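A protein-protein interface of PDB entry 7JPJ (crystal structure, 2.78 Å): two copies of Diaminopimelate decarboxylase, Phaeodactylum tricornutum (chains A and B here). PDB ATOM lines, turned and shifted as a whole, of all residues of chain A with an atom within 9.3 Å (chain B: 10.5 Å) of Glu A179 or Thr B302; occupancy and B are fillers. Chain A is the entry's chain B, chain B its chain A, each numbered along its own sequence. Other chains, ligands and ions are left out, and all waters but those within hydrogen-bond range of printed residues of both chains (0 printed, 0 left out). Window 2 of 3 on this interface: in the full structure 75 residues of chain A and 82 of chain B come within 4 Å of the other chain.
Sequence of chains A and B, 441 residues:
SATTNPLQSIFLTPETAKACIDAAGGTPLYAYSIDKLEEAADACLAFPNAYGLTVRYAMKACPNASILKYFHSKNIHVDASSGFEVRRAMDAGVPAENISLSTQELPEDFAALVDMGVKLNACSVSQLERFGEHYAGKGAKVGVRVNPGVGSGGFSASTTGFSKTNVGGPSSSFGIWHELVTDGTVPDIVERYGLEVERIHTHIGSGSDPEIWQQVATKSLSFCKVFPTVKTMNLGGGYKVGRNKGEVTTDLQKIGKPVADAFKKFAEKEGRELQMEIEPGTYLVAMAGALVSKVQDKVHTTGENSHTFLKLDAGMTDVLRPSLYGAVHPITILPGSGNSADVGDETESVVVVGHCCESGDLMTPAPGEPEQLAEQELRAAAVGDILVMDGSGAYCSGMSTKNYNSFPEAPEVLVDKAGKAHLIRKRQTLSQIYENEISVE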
ATOM      1  N   VAL A 125     -12.052 -24.370 -10.192  1.00  0.00           N
ATOM      2  CA  VAL A 125     -11.217 -25.373 -10.848  1.00  0.00           C
ATOM      3  C   VAL A 125      -9.981 -24.716 -11.448  1.00  0.00           C
ATOM      4  O   VAL A 125      -8.869 -25.257 -11.371  1.00  0.00           O
ATOM      5  CB  VAL A 125     -12.036 -26.131 -11.910  1.00  0.00           C
ATOM      6  CG1 VAL A 125     -11.139 -26.991 -12.779  1.00  0.00           C
ATOM      7  CG2 VAL A 125     -13.106 -26.979 -11.244  1.00  0.00           C
ATOM      8  N   VAL A 146     -16.034 -24.855  -1.379  1.00  0.00           N
ATOM      9  CA  VAL A 146     -17.060 -25.630  -2.067  1.00  0.00           C
ATOM     10  C   VAL A 146     -18.384 -24.884  -2.009  1.00  0.00           C
ATOM     11  O   VAL A 146     -18.823 -24.464  -0.930  1.00  0.00           O
ATOM     12  CB  VAL A 146     -17.200 -27.034  -1.454  1.00  0.00           C
ATOM     13  CG1 VAL A 146     -18.327 -27.799  -2.132  1.00  0.00           C
ATOM     14  CG2 VAL A 146     -15.888 -27.790  -1.566  1.00  0.00           C
ATOM     15  N   ASN A 147     -19.019 -24.718  -3.175  1.00  0.00           N
ATOM     16  CA  ASN A 147     -20.412 -24.300  -3.258  1.00  0.00           C
ATOM     17  C   ASN A 147     -21.276 -25.509  -2.921  1.00  0.00           C
ATOM     18  O   ASN A 147     -21.384 -26.434  -3.735  1.00  0.00           O
ATOM     19  CB  ASN A 147     -20.737 -23.757  -4.653  1.00  0.00           C
ATOM     20  CG  ASN A 147     -22.147 -23.178  -4.757  1.00  0.00           C
ATOM     21  OD1 ASN A 147     -23.079 -23.635  -4.099  1.00  0.00           O
ATOM     22  ND2 ASN A 147     -22.301 -22.165  -5.601  1.00  0.00           N
ATOM     23  N   PRO A 148     -21.904 -25.544  -1.742  1.00  0.00           N
ATOM     24  CA  PRO A 148     -22.609 -26.766  -1.320  1.00  0.00           C
ATOM     25  C   PRO A 148     -23.810 -27.116  -2.179  1.00  0.00           C
ATOM     26  O   PRO A 148     -24.343 -28.222  -2.038  1.00  0.00           O
ATOM     27  CB  PRO A 148     -23.038 -26.447   0.121  1.00  0.00           C
ATOM     28  CG  PRO A 148     -22.212 -25.263   0.530  1.00  0.00           C
ATOM     29  CD  PRO A 148     -21.980 -24.487  -0.722  1.00  0.00           C
ATOM     30  N   GLY A 149     -24.245 -26.228  -3.066  1.00  0.00           N
ATOM     31  CA  GLY A 149     -25.428 -26.450  -3.862  1.00  0.00           C
ATOM     32  C   GLY A 149     -26.662 -25.742  -3.353  1.00  0.00           C
ATOM     33  O   GLY A 149     -27.679 -25.716  -4.057  1.00  0.00           O
ATOM     34  N   GLY A 169     -25.443 -21.796  -4.015  1.00  0.00           N
ATOM     35  CA  GLY A 169     -26.488 -22.282  -4.884  1.00  0.00           C
ATOM     36  C   GLY A 169     -26.153 -22.099  -6.351  1.00  0.00           C
ATOM     37  O   GLY A 169     -25.037 -21.717  -6.716  1.00  0.00           O
ATOM     38  N   PRO A 170     -27.125 -22.364  -7.230  1.00  0.00           N
ATOM     39  CA  PRO A 170     -26.863 -22.241  -8.671  1.00  0.00           C
ATOM     40  C   PRO A 170     -26.717 -20.806  -9.143  1.00  0.00           C
ATOM     41  O   PRO A 170     -26.313 -20.593 -10.293  1.00  0.00           O
ATOM     42  CB  PRO A 170     -28.084 -22.915  -9.306  1.00  0.00           C
ATOM     43  CG  PRO A 170     -29.171 -22.702  -8.307  1.00  0.00           C
ATOM     44  CD  PRO A 170     -28.516 -22.763  -6.951  1.00  0.00           C
ATOM     45  N   SER A 171     -27.024 -19.824  -8.297  1.00  0.00           N
ATOM     46  CA  SER A 171     -26.908 -18.416  -8.648  1.00  0.00           C
ATOM     47  C   SER A 171     -25.558 -17.815  -8.282  1.00  0.00           C
ATOM     48  O   SER A 171     -25.241 -16.719  -8.755  1.00  0.00           O
ATOM     49  CB  SER A 171     -28.010 -17.607  -7.958  1.00  0.00           C
ATOM     50  OG  SER A 171     -29.168 -17.526  -8.765  1.00  0.00           O
ATOM     51  N   SER A 172     -24.768 -18.493  -7.456  1.00  0.00           N
ATOM     52  CA  SER A 172     -23.524 -17.936  -6.948  1.00  0.00           C
ATOM     53  C   SER A 172     -22.333 -18.374  -7.789  1.00  0.00           C
ATOM     54  O   SER A 172     -22.331 -19.452  -8.387  1.00  0.00           O
ATOM     55  CB  SER A 172     -23.297 -18.359  -5.497  1.00  0.00           C
ATOM     56  OG  SER A 172     -22.446 -17.445  -4.831  1.00  0.00           O
ATOM     57  N   GLY A 175     -18.318 -21.232  -4.775  1.00  0.00           N
ATOM     58  CA  GLY A 175     -17.035 -21.206  -5.451  1.00  0.00           C
ATOM     59  C   GLY A 175     -16.985 -22.375  -6.419  1.00  0.00           C
ATOM     60  O   GLY A 175     -17.437 -22.254  -7.558  1.00  0.00           O
ATOM     61  N   ILE A 176     -16.459 -23.513  -5.971  1.00  0.00           N
ATOM     62  CA  ILE A 176     -16.464 -24.722  -6.789  1.00  0.00           C
ATOM     63  C   ILE A 176     -17.811 -25.413  -6.644  1.00  0.00           C
ATOM     64  O   ILE A 176     -18.260 -25.698  -5.527  1.00  0.00           O
ATOM     65  CB  ILE A 176     -15.317 -25.663  -6.392  1.00  0.00           C
ATOM     66  CG1 ILE A 176     -13.966 -25.007  -6.666  1.00  0.00           C
ATOM     67  CG2 ILE A 176     -15.433 -26.980  -7.147  1.00  0.00           C
ATOM     68  CD1 ILE A 176     -12.788 -25.944  -6.521  1.00  0.00           C
ATOM     69  N   TRP A 177     -18.459 -25.686  -7.773  1.00  0.00           N
ATOM     70  CA  TRP A 177     -19.757 -26.346  -7.753  1.00  0.00           C
ATOM     71  C   TRP A 177     -19.623 -27.747  -7.169  1.00  0.00           C
ATOM     72  O   TRP A 177     -18.707 -28.497  -7.523  1.00  0.00           O
ATOM     73  CB  TRP A 177     -20.334 -26.401  -9.168  1.00  0.00           C
ATOM     74  CG  TRP A 177     -21.775 -26.816  -9.246  1.00  0.00           C
ATOM     75  CD1 TRP A 177     -22.288 -27.849  -9.974  1.00  0.00           C
ATOM     76  CD2 TRP A 177     -22.889 -26.201  -8.585  1.00  0.00           C
ATOM     77  NE1 TRP A 177     -23.649 -27.919  -9.804  1.00  0.00           N
ATOM     78  CE2 TRP A 177     -24.043 -26.919  -8.956  1.00  0.00           C
ATOM     79  CE3 TRP A 177     -23.023 -25.116  -7.713  1.00  0.00           C
ATOM     80  CZ2 TRP A 177     -25.312 -26.588  -8.486  1.00  0.00           C
ATOM     81  CZ3 TRP A 177     -24.284 -24.790  -7.249  1.00  0.00           C
ATOM     82  CH2 TRP A 177     -25.411 -25.524  -7.637  1.00  0.00           C
ATOM     83  N   HIS A 178     -20.545 -28.095  -6.266  1.00  0.00           N
ATOM     84  CA  HIS A 178     -20.433 -29.349  -5.525  1.00  0.00           C
ATOM     85  C   HIS A 178     -20.460 -30.561  -6.443  1.00  0.00           C
ATOM     86  O   HIS A 178     -19.884 -31.603  -6.110  1.00  0.00           O
ATOM     87  CB  HIS A 178     -21.557 -29.451  -4.494  1.00  0.00           C
ATOM     88  CG  HIS A 178     -22.897 -29.759  -5.090  1.00  0.00           C
ATOM     89  ND1 HIS A 178     -23.561 -28.884  -5.923  1.00  0.00           N
ATOM     90  CD2 HIS A 178     -23.698 -30.844  -4.969  1.00  0.00           C
ATOM     91  CE1 HIS A 178     -24.711 -29.417  -6.293  1.00  0.00           C
ATOM     92  NE2 HIS A 178     -24.818 -30.606  -5.728  1.00  0.00           N
ATOM     93  N   GLU A 179     -21.121 -30.454  -7.597  1.00  0.00           N
ATOM     94  CA  GLU A 179     -21.205 -31.601  -8.491  1.00  0.00           C
ATOM     95  C   GLU A 179     -19.872 -31.926  -9.148  1.00  0.00           C
ATOM     96  O   GLU A 179     -19.677 -33.062  -9.589  1.00  0.00           O
ATOM     97  CB  GLU A 179     -22.276 -31.375  -9.555  1.00  0.00           C
ATOM     98  CG  GLU A 179     -23.688 -31.582  -9.035  1.00  0.00           C
ATOM     99  CD  GLU A 179     -24.747 -31.190 -10.044  1.00  0.00           C
ATOM    100  OE1 GLU A 179     -25.947 -31.212  -9.689  1.00  0.00           O
ATOM    101  OE2 GLU A 179     -24.378 -30.866 -11.196  1.00  0.00           O
ATOM    102  N   LEU A 180     -18.954 -30.963  -9.224  1.00  0.00           N
ATOM    103  CA  LEU A 180     -17.608 -31.267  -9.688  1.00  0.00           C
ATOM    104  C   LEU A 180     -16.786 -31.987  -8.629  1.00  0.00           C
ATOM    105  O   LEU A 180     -15.770 -32.608  -8.963  1.00  0.00           O
ATOM    106  CB  LEU A 180     -16.896 -29.985 -10.125  1.00  0.00           C
ATOM    107  CG  LEU A 180     -17.467 -29.334 -11.388  1.00  0.00           C
ATOM    108  CD1 LEU A 180     -17.053 -27.872 -11.488  1.00  0.00           C
ATOM    109  CD2 LEU A 180     -17.062 -30.104 -12.636  1.00  0.00           C
ATOM    110  N   VAL A 181     -17.198 -31.922  -7.365  1.00  0.00           N
ATOM    111  CA  VAL A 181     -16.538 -32.717  -6.338  1.00  0.00           C
ATOM    112  C   VAL A 181     -17.092 -34.135  -6.327  1.00  0.00           C
ATOM    113  O   VAL A 181     -16.337 -35.109  -6.238  1.00  0.00           O
ATOM    114  CB  VAL A 181     -16.684 -32.044  -4.960  1.00  0.00           C
ATOM    115  CG1 VAL A 181     -16.120 -32.944  -3.868  1.00  0.00           C
ATOM    116  CG2 VAL A 181     -15.991 -30.691  -4.951  1.00  0.00           C
ATOM    117  N   THR A 182     -18.412 -34.272  -6.432  1.00  0.00           N
ATOM    118  CA  THR A 182     -19.063 -35.570  -6.321  1.00  0.00           C
ATOM    119  C   THR A 182     -19.000 -36.390  -7.603  1.00  0.00           C
ATOM    120  O   THR A 182     -19.504 -37.517  -7.617  1.00  0.00           O
ATOM    121  CB  THR A 182     -20.526 -35.391  -5.896  1.00  0.00           C
ATOM    122  OG1 THR A 182     -21.265 -34.770  -6.957  1.00  0.00           O
ATOM    123  CG2 THR A 182     -20.613 -34.524  -4.646  1.00  0.00           C
ATOM    124  N   ASP A 183     -18.406 -35.864  -8.679  1.00  0.00           N
ATOM    125  CA  ASP A 183     -18.211 -36.644  -9.898  1.00  0.00           C
ATOM    126  C   ASP A 183     -16.733 -36.861 -10.215  1.00  0.00           C
ATOM    127  O   ASP A 183     -16.385 -37.167 -11.360  1.00  0.00           O
ATOM    128  CB  ASP A 183     -18.959 -36.020 -11.090  1.00  0.00           C
ATOM    129  CG  ASP A 183     -18.307 -34.747 -11.637  1.00  0.00           C
ATOM    130  OD1 ASP A 183     -17.283 -34.282 -11.093  1.00  0.00           O
ATOM    131  OD2 ASP A 183     -18.866 -34.165 -12.593  1.00  0.00           O
ATOM    132  N   GLY A 184     -15.860 -36.717  -9.221  1.00  0.00           N
ATOM    133  CA  GLY A 184     -14.468 -37.067  -9.366  1.00  0.00           C
ATOM    134  C   GLY A 184     -13.576 -35.983  -9.932  1.00  0.00           C
ATOM    135  O   GLY A 184     -12.355 -36.061  -9.760  1.00  0.00           O
ATOM    136  N   THR A 185     -14.147 -34.961 -10.577  1.00  0.00           N
ATOM    137  CA  THR A 185     -13.328 -33.974 -11.280  1.00  0.00           C
ATOM    138  C   THR A 185     -12.321 -33.312 -10.343  1.00  0.00           C
ATOM    139  O   THR A 185     -11.116 -33.297 -10.621  1.00  0.00           O
ATOM    140  CB  THR A 185     -14.219 -32.924 -11.951  1.00  0.00           C
ATOM    141  OG1 THR A 185     -14.918 -33.521 -13.052  1.00  0.00           O
ATOM    142  CG2 THR A 185     -13.383 -31.761 -12.464  1.00  0.00           C
ATOM    143  N   VAL A 186     -12.789 -32.771  -9.223  1.00  0.00           N
ATOM    144  CA  VAL A 186     -11.893 -32.121  -8.267  1.00  0.00           C
ATOM    145  C   VAL A 186     -10.993 -33.157  -7.596  1.00  0.00           C
ATOM    146  O   VAL A 186      -9.795 -32.892  -7.423  1.00  0.00           O
ATOM    147  CB  VAL A 186     -12.679 -31.299  -7.233  1.00  0.00           C
ATOM    148  CG1 VAL A 186     -11.736 -30.710  -6.196  1.00  0.00           C
ATOM    149  CG2 VAL A 186     -13.473 -30.201  -7.924  1.00  0.00           C
ATOM    150  N   PRO A 187     -11.496 -34.335  -7.193  1.00  0.00           N
ATOM    151  CA  PRO A 187     -10.572 -35.376  -6.711  1.00  0.00           C
ATOM    152  C   PRO A 187      -9.453 -35.716  -7.686  1.00  0.00           C
ATOM    153  O   PRO A 187      -8.302 -35.849  -7.259  1.00  0.00           O
ATOM    154  CB  PRO A 187     -11.502 -36.572  -6.474  1.00  0.00           C
ATOM    155  CG  PRO A 187     -12.771 -35.956  -6.072  1.00  0.00           C
ATOM    156  CD  PRO A 187     -12.898 -34.701  -6.900  1.00  0.00           C
ATOM    157  N   PHE A 223     -18.542 -32.855   2.706  1.00  0.00           N
ATOM    158  CA  PHE A 223     -17.483 -32.720   1.717  1.00  0.00           C
ATOM    159  C   PHE A 223     -16.106 -33.043   2.277  1.00  0.00           C
ATOM    160  O   PHE A 223     -15.209 -33.400   1.505  1.00  0.00           O
ATOM    161  CB  PHE A 223     -17.489 -31.310   1.122  1.00  0.00           C
ATOM    162  CG  PHE A 223     -18.726 -31.007   0.331  1.00  0.00           C
ATOM    163  CD1 PHE A 223     -18.883 -31.515  -0.948  1.00  0.00           C
ATOM    164  CD2 PHE A 223     -19.736 -30.232   0.870  1.00  0.00           C
ATOM    165  CE1 PHE A 223     -20.025 -31.249  -1.679  1.00  0.00           C
ATOM    166  CE2 PHE A 223     -20.880 -29.960   0.144  1.00  0.00           C
ATOM    167  CZ  PHE A 223     -21.025 -30.470  -1.132  1.00  0.00           C
ATOM    168  N   VAL B 299     -16.576 -19.911 -14.624  1.00  0.00           N
ATOM    169  CA  VAL B 299     -17.102 -21.010 -13.823  1.00  0.00           C
ATOM    170  C   VAL B 299     -18.541 -21.298 -14.238  1.00  0.00           C
ATOM    171  O   VAL B 299     -19.204 -20.483 -14.882  1.00  0.00           O
ATOM    172  CB  VAL B 299     -17.027 -20.709 -12.311  1.00  0.00           C
ATOM    173  CG1 VAL B 299     -15.602 -20.363 -11.914  1.00  0.00           C
ATOM    174  CG2 VAL B 299     -17.970 -19.579 -11.950  1.00  0.00           C
ATOM    175  N   HIS B 300     -19.023 -22.480 -13.853  1.00  0.00           N
ATOM    176  CA  HIS B 300     -20.351 -22.933 -14.240  1.00  0.00           C
ATOM    177  C   HIS B 300     -21.093 -23.515 -13.044  1.00  0.00           C
ATOM    178  O   HIS B 300     -20.486 -23.994 -12.082  1.00  0.00           O
ATOM    179  CB  HIS B 300     -20.288 -23.997 -15.353  1.00  0.00           C
ATOM    180  CG  HIS B 300     -19.310 -23.683 -16.442  1.00  0.00           C
ATOM    181  ND1 HIS B 300     -19.647 -22.940 -17.555  1.00  0.00           N
ATOM    182  CD2 HIS B 300     -18.008 -24.020 -16.595  1.00  0.00           C
ATOM    183  CE1 HIS B 300     -18.593 -22.830 -18.344  1.00  0.00           C
ATOM    184  NE2 HIS B 300     -17.584 -23.475 -17.785  1.00  0.00           N
ATOM    185  N   THR B 301     -22.421 -23.463 -13.123  1.00  0.00           N
ATOM    186  CA  THR B 301     -23.310 -24.206 -12.246  1.00  0.00           C
ATOM    187  C   THR B 301     -24.219 -25.074 -13.108  1.00  0.00           C
ATOM    188  O   THR B 301     -24.357 -24.850 -14.313  1.00  0.00           O
ATOM    189  CB  THR B 301     -24.155 -23.277 -11.358  1.00  0.00           C
ATOM    190  OG1 THR B 301     -24.666 -22.194 -12.143  1.00  0.00           O
ATOM    191  CG2 THR B 301     -23.319 -22.716 -10.222  1.00  0.00           C
ATOM    192  N   THR B 302     -24.830 -26.080 -12.488  1.00  0.00           N
ATOM    193  CA  THR B 302     -25.734 -26.978 -13.193  1.00  0.00           C
ATOM    194  C   THR B 302     -27.097 -26.982 -12.514  1.00  0.00           C
ATOM    195  O   THR B 302     -27.303 -26.365 -11.466  1.00  0.00           O
ATOM    196  CB  THR B 302     -25.187 -28.409 -13.255  1.00  0.00           C
ATOM    197  OG1 THR B 302     -25.491 -29.086 -12.030  1.00  0.00           O
ATOM    198  CG2 THR B 302     -23.681 -28.405 -13.473  1.00  0.00           C
ATOM    199  N   GLY B 303     -28.034 -27.693 -13.134  1.00  0.00           N
ATOM    200  CA  GLY B 303     -29.373 -27.795 -12.596  1.00  0.00           C
ATOM    201  C   GLY B 303     -30.218 -26.572 -12.902  1.00  0.00           C
ATOM    202  O   GLY B 303     -29.915 -25.761 -13.783  1.00  0.00           O
ATOM    203  N   GLU B 304     -31.306 -26.448 -12.148  1.00  0.00           N
ATOM    204  CA  GLU B 304     -32.226 -25.335 -12.328  1.00  0.00           C
ATOM    205  C   GLU B 304     -31.561 -24.019 -11.941  1.00  0.00           C
ATOM    206  O   GLU B 304     -30.750 -23.956 -11.011  1.00  0.00           O
ATOM    207  CB  GLU B 304     -33.488 -25.548 -11.493  1.00  0.00           C
ATOM    208  CG  GLU B 304     -33.217 -26.095 -10.095  1.00  0.00           C
ATOM    209  CD  GLU B 304     -34.328 -25.763  -9.115  1.00  0.00           C
ATOM    210  OE1 GLU B 304     -34.943 -24.684  -9.258  1.00  0.00           O
ATOM    211  OE2 GLU B 304     -34.583 -26.575  -8.199  1.00  0.00           O
ATOM    212  N   ASN B 305     -31.922 -22.958 -12.670  1.00  0.00           N
ATOM    213  CA  ASN B 305     -31.383 -21.611 -12.456  1.00  0.00           C
ATOM    214  C   ASN B 305     -29.860 -21.587 -12.515  1.00  0.00           C
ATOM    215  O   ASN B 305     -29.215 -20.784 -11.837  1.00  0.00           O
ATOM    216  CB  ASN B 305     -31.870 -21.013 -11.132  1.00  0.00           C
ATOM    217  CG  ASN B 305     -33.352 -21.223 -10.905  1.00  0.00           C
ATOM    218  OD1 ASN B 305     -33.895 -22.285 -11.210  1.00  0.00           O
ATOM    219  ND2 ASN B 305     -34.017 -20.208 -10.361  1.00  0.00           N
ATOM    220  N   SER B 306     -29.272 -22.462 -13.324  1.00  0.00           N
ATOM    221  CA  SER B 306     -27.827 -22.485 -13.465  1.00  0.00           C
ATOM    222  C   SER B 306     -27.375 -21.469 -14.509  1.00  0.00           C
ATOM    223  O   SER B 306     -28.130 -21.065 -15.396  1.00  0.00           O
ATOM    224  CB  SER B 306     -27.343 -23.881 -13.847  1.00  0.00           C
ATOM    225  OG  SER B 306     -27.925 -24.318 -15.062  1.00  0.00           O
ATOM    226  N   HIS B 307     -26.119 -21.053 -14.389  1.00  0.00           N
ATOM    227  CA  HIS B 307     -25.569 -20.016 -15.243  1.00  0.00           C
ATOM    228  C   HIS B 307     -24.124 -20.346 -15.578  1.00  0.00           C
ATOM    229  O   HIS B 307     -23.502 -21.223 -14.972  1.00  0.00           O
ATOM    230  CB  HIS B 307     -25.648 -18.636 -14.577  1.00  0.00           C
ATOM    231  CG  HIS B 307     -27.043 -18.175 -14.300  1.00  0.00           C
ATOM    232  ND1 HIS B 307     -27.817 -18.704 -13.289  1.00  0.00           N
ATOM    233  CD2 HIS B 307     -27.803 -17.227 -14.898  1.00  0.00           C
ATOM    234  CE1 HIS B 307     -28.995 -18.108 -13.282  1.00  0.00           C
ATOM    235  NE2 HIS B 307     -29.013 -17.207 -14.247  1.00  0.00           N
ATOM    236  N   THR B 308     -23.600 -19.628 -16.566  1.00  0.00           N
ATOM    237  CA  THR B 308     -22.172 -19.561 -16.833  1.00  0.00           C
ATOM    238  C   THR B 308     -21.689 -18.177 -16.427  1.00  0.00           C
ATOM    239  O   THR B 308     -22.252 -17.169 -16.861  1.00  0.00           O
ATOM    240  CB  THR B 308     -21.867 -19.831 -18.308  1.00  0.00           C
ATOM    241  OG1 THR B 308     -22.005 -21.232 -18.573  1.00  0.00           O
ATOM    242  CG2 THR B 308     -20.451 -19.393 -18.654  1.00  0.00           C
ATOM    243  N   PHE B 309     -20.664 -18.133 -15.579  1.00  0.00           N
ATOM    244  CA  PHE B 309     -20.193 -16.893 -14.978  1.00  0.00           C
ATOM    245  C   PHE B 309     -18.842 -16.502 -15.564  1.00  0.00           C
ATOM    246  O   PHE B 309     -17.914 -17.317 -15.594  1.00  0.00           O
ATOM    247  CB  PHE B 309     -20.074 -17.030 -13.458  1.00  0.00           C
ATOM    248  CG  PHE B 309     -21.378 -17.301 -12.764  1.00  0.00           C
ATOM    249  CD1 PHE B 309     -21.875 -18.590 -12.667  1.00  0.00           C
ATOM    250  CD2 PHE B 309     -22.104 -16.267 -12.195  1.00  0.00           C
ATOM    251  CE1 PHE B 309     -23.073 -18.837 -12.022  1.00  0.00           C
ATOM    252  CE2 PHE B 309     -23.301 -16.512 -11.550  1.00  0.00           C
ATOM    253  CZ  PHE B 309     -23.786 -17.796 -11.463  1.00  0.00           C
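Among the printed residues, pairs that only touch across the chains: Ser A171 with Phe B309 (3.3 Å), Pro A170 with Glu B304 (3.3 Å), Trp A177 with Thr B301 (3.5 Å), Ser A172 with Phe B309 (3.8 Å), Trp A177 with His B300 (3.8 Å), Pro A170 with His B307 (3.8 Å), Ser A172 with Thr B301 (3.9 Å), Pro A170 with Phe B309 (3.9 Å) and Pro A170 with Ser B306 (3.99 Å).
A ring nitrogen (ND1) of His B300 lies within hydrogen-bond range of the side-chain hydroxyl (OG1) of Thr B308, at 3.1 Å. The side-chain hydroxyl (OG1) of Thr B301 is in hydrogen-bond range of the backbone NH (N) of His B307 (2.9 Å). O of Gly B303 is in hydrogen-bond range of OG of Ser B306, 2.8 Å away. The side-chain carboxylate (OE1) of Glu B304 lies close to the side-chain amide oxygen (OD1) of Asn B305, 3.3 Å away. O of Asn B305 sits at hydrogen-bond distance from ND1 of His B307 (2.9 Å). The side-chain carboxylate (OE2) of Glu A179 sits at hydrogen-bond distance from the indole nitrogen (NE1) of Trp A177, 3.3 Å away.
O of Pro A170 is in hydrogen-bond range of OG1 of Thr B301 (2.9 Å). NE1 of Trp A177 sits at hydrogen-bond distance from OG1 of Thr B302 (3.1 Å). The side-chain hydroxyl (OG1) of Thr B302 lies close to the side-chain carboxylate (OE1) of Glu A179, 3.2 Å away. The backbone carbonyl oxygen (O) of Pro A170 sits close to the backbone carbonyl oxygen (O) of Asn B305, 3.3 Å away.
No position is printed for both chains. Of the 13 pairs that touch across the chains among the printed residues, none has its exchanged pair printed and touching as well.
Of the 11 printed residues of chain B, 8 touch a printed residue of chain A. Printed residues of chain B that touch a printed residue of chain A: His B300, Thr B301, Thr B302, Glu B304, Asn B305, Ser B306, His B307 and Phe B309. Hydrophobic or aromatic side chains of chain B within 4 Å of the printed part of chain A: His B307 and Phe B309. Printed residues of chain A that touch a printed residue of chain B: Pro A170, Ser A171, Ser A172, Trp A177 and Glu A179.
Of chain B, only Thr B302 (2.3 Å) comes within 4 Å of Glu A179. Of chain A, only Trp A177 (3.1 Å) and Glu A179 (2.3 Å) come within 4 Å of Thr B302. Printed residues of chain B within 4 Å of Trp A177: His B300, Thr B301 and Thr B302. No residue of chain B comes within 4 Å of His A178. No residue of chain B comes within 4 Å of Leu A180. No residue of chain B comes within 4 Å of Thr A182. Asp A183 touches none of the printed residues of chain B. No residue of chain A comes within 4 Å of Gly B303. Of the printed residues of chain A, Phe B309 touches Pro A170, Ser A171 and Ser A172. Of the printed residues of chain B, Ser A171 touches Phe B309 (3.3 Å). Val A186 touches none of the printed residues of chain B. Val A146 touches none of the printed residues of chain B. The nearest residue of chain B that does not touch Glu A179 is Gly B303 (5.2 Å). The nearest residue of chain A that does not touch Thr B302 is Pro A170 (4.1 Å).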
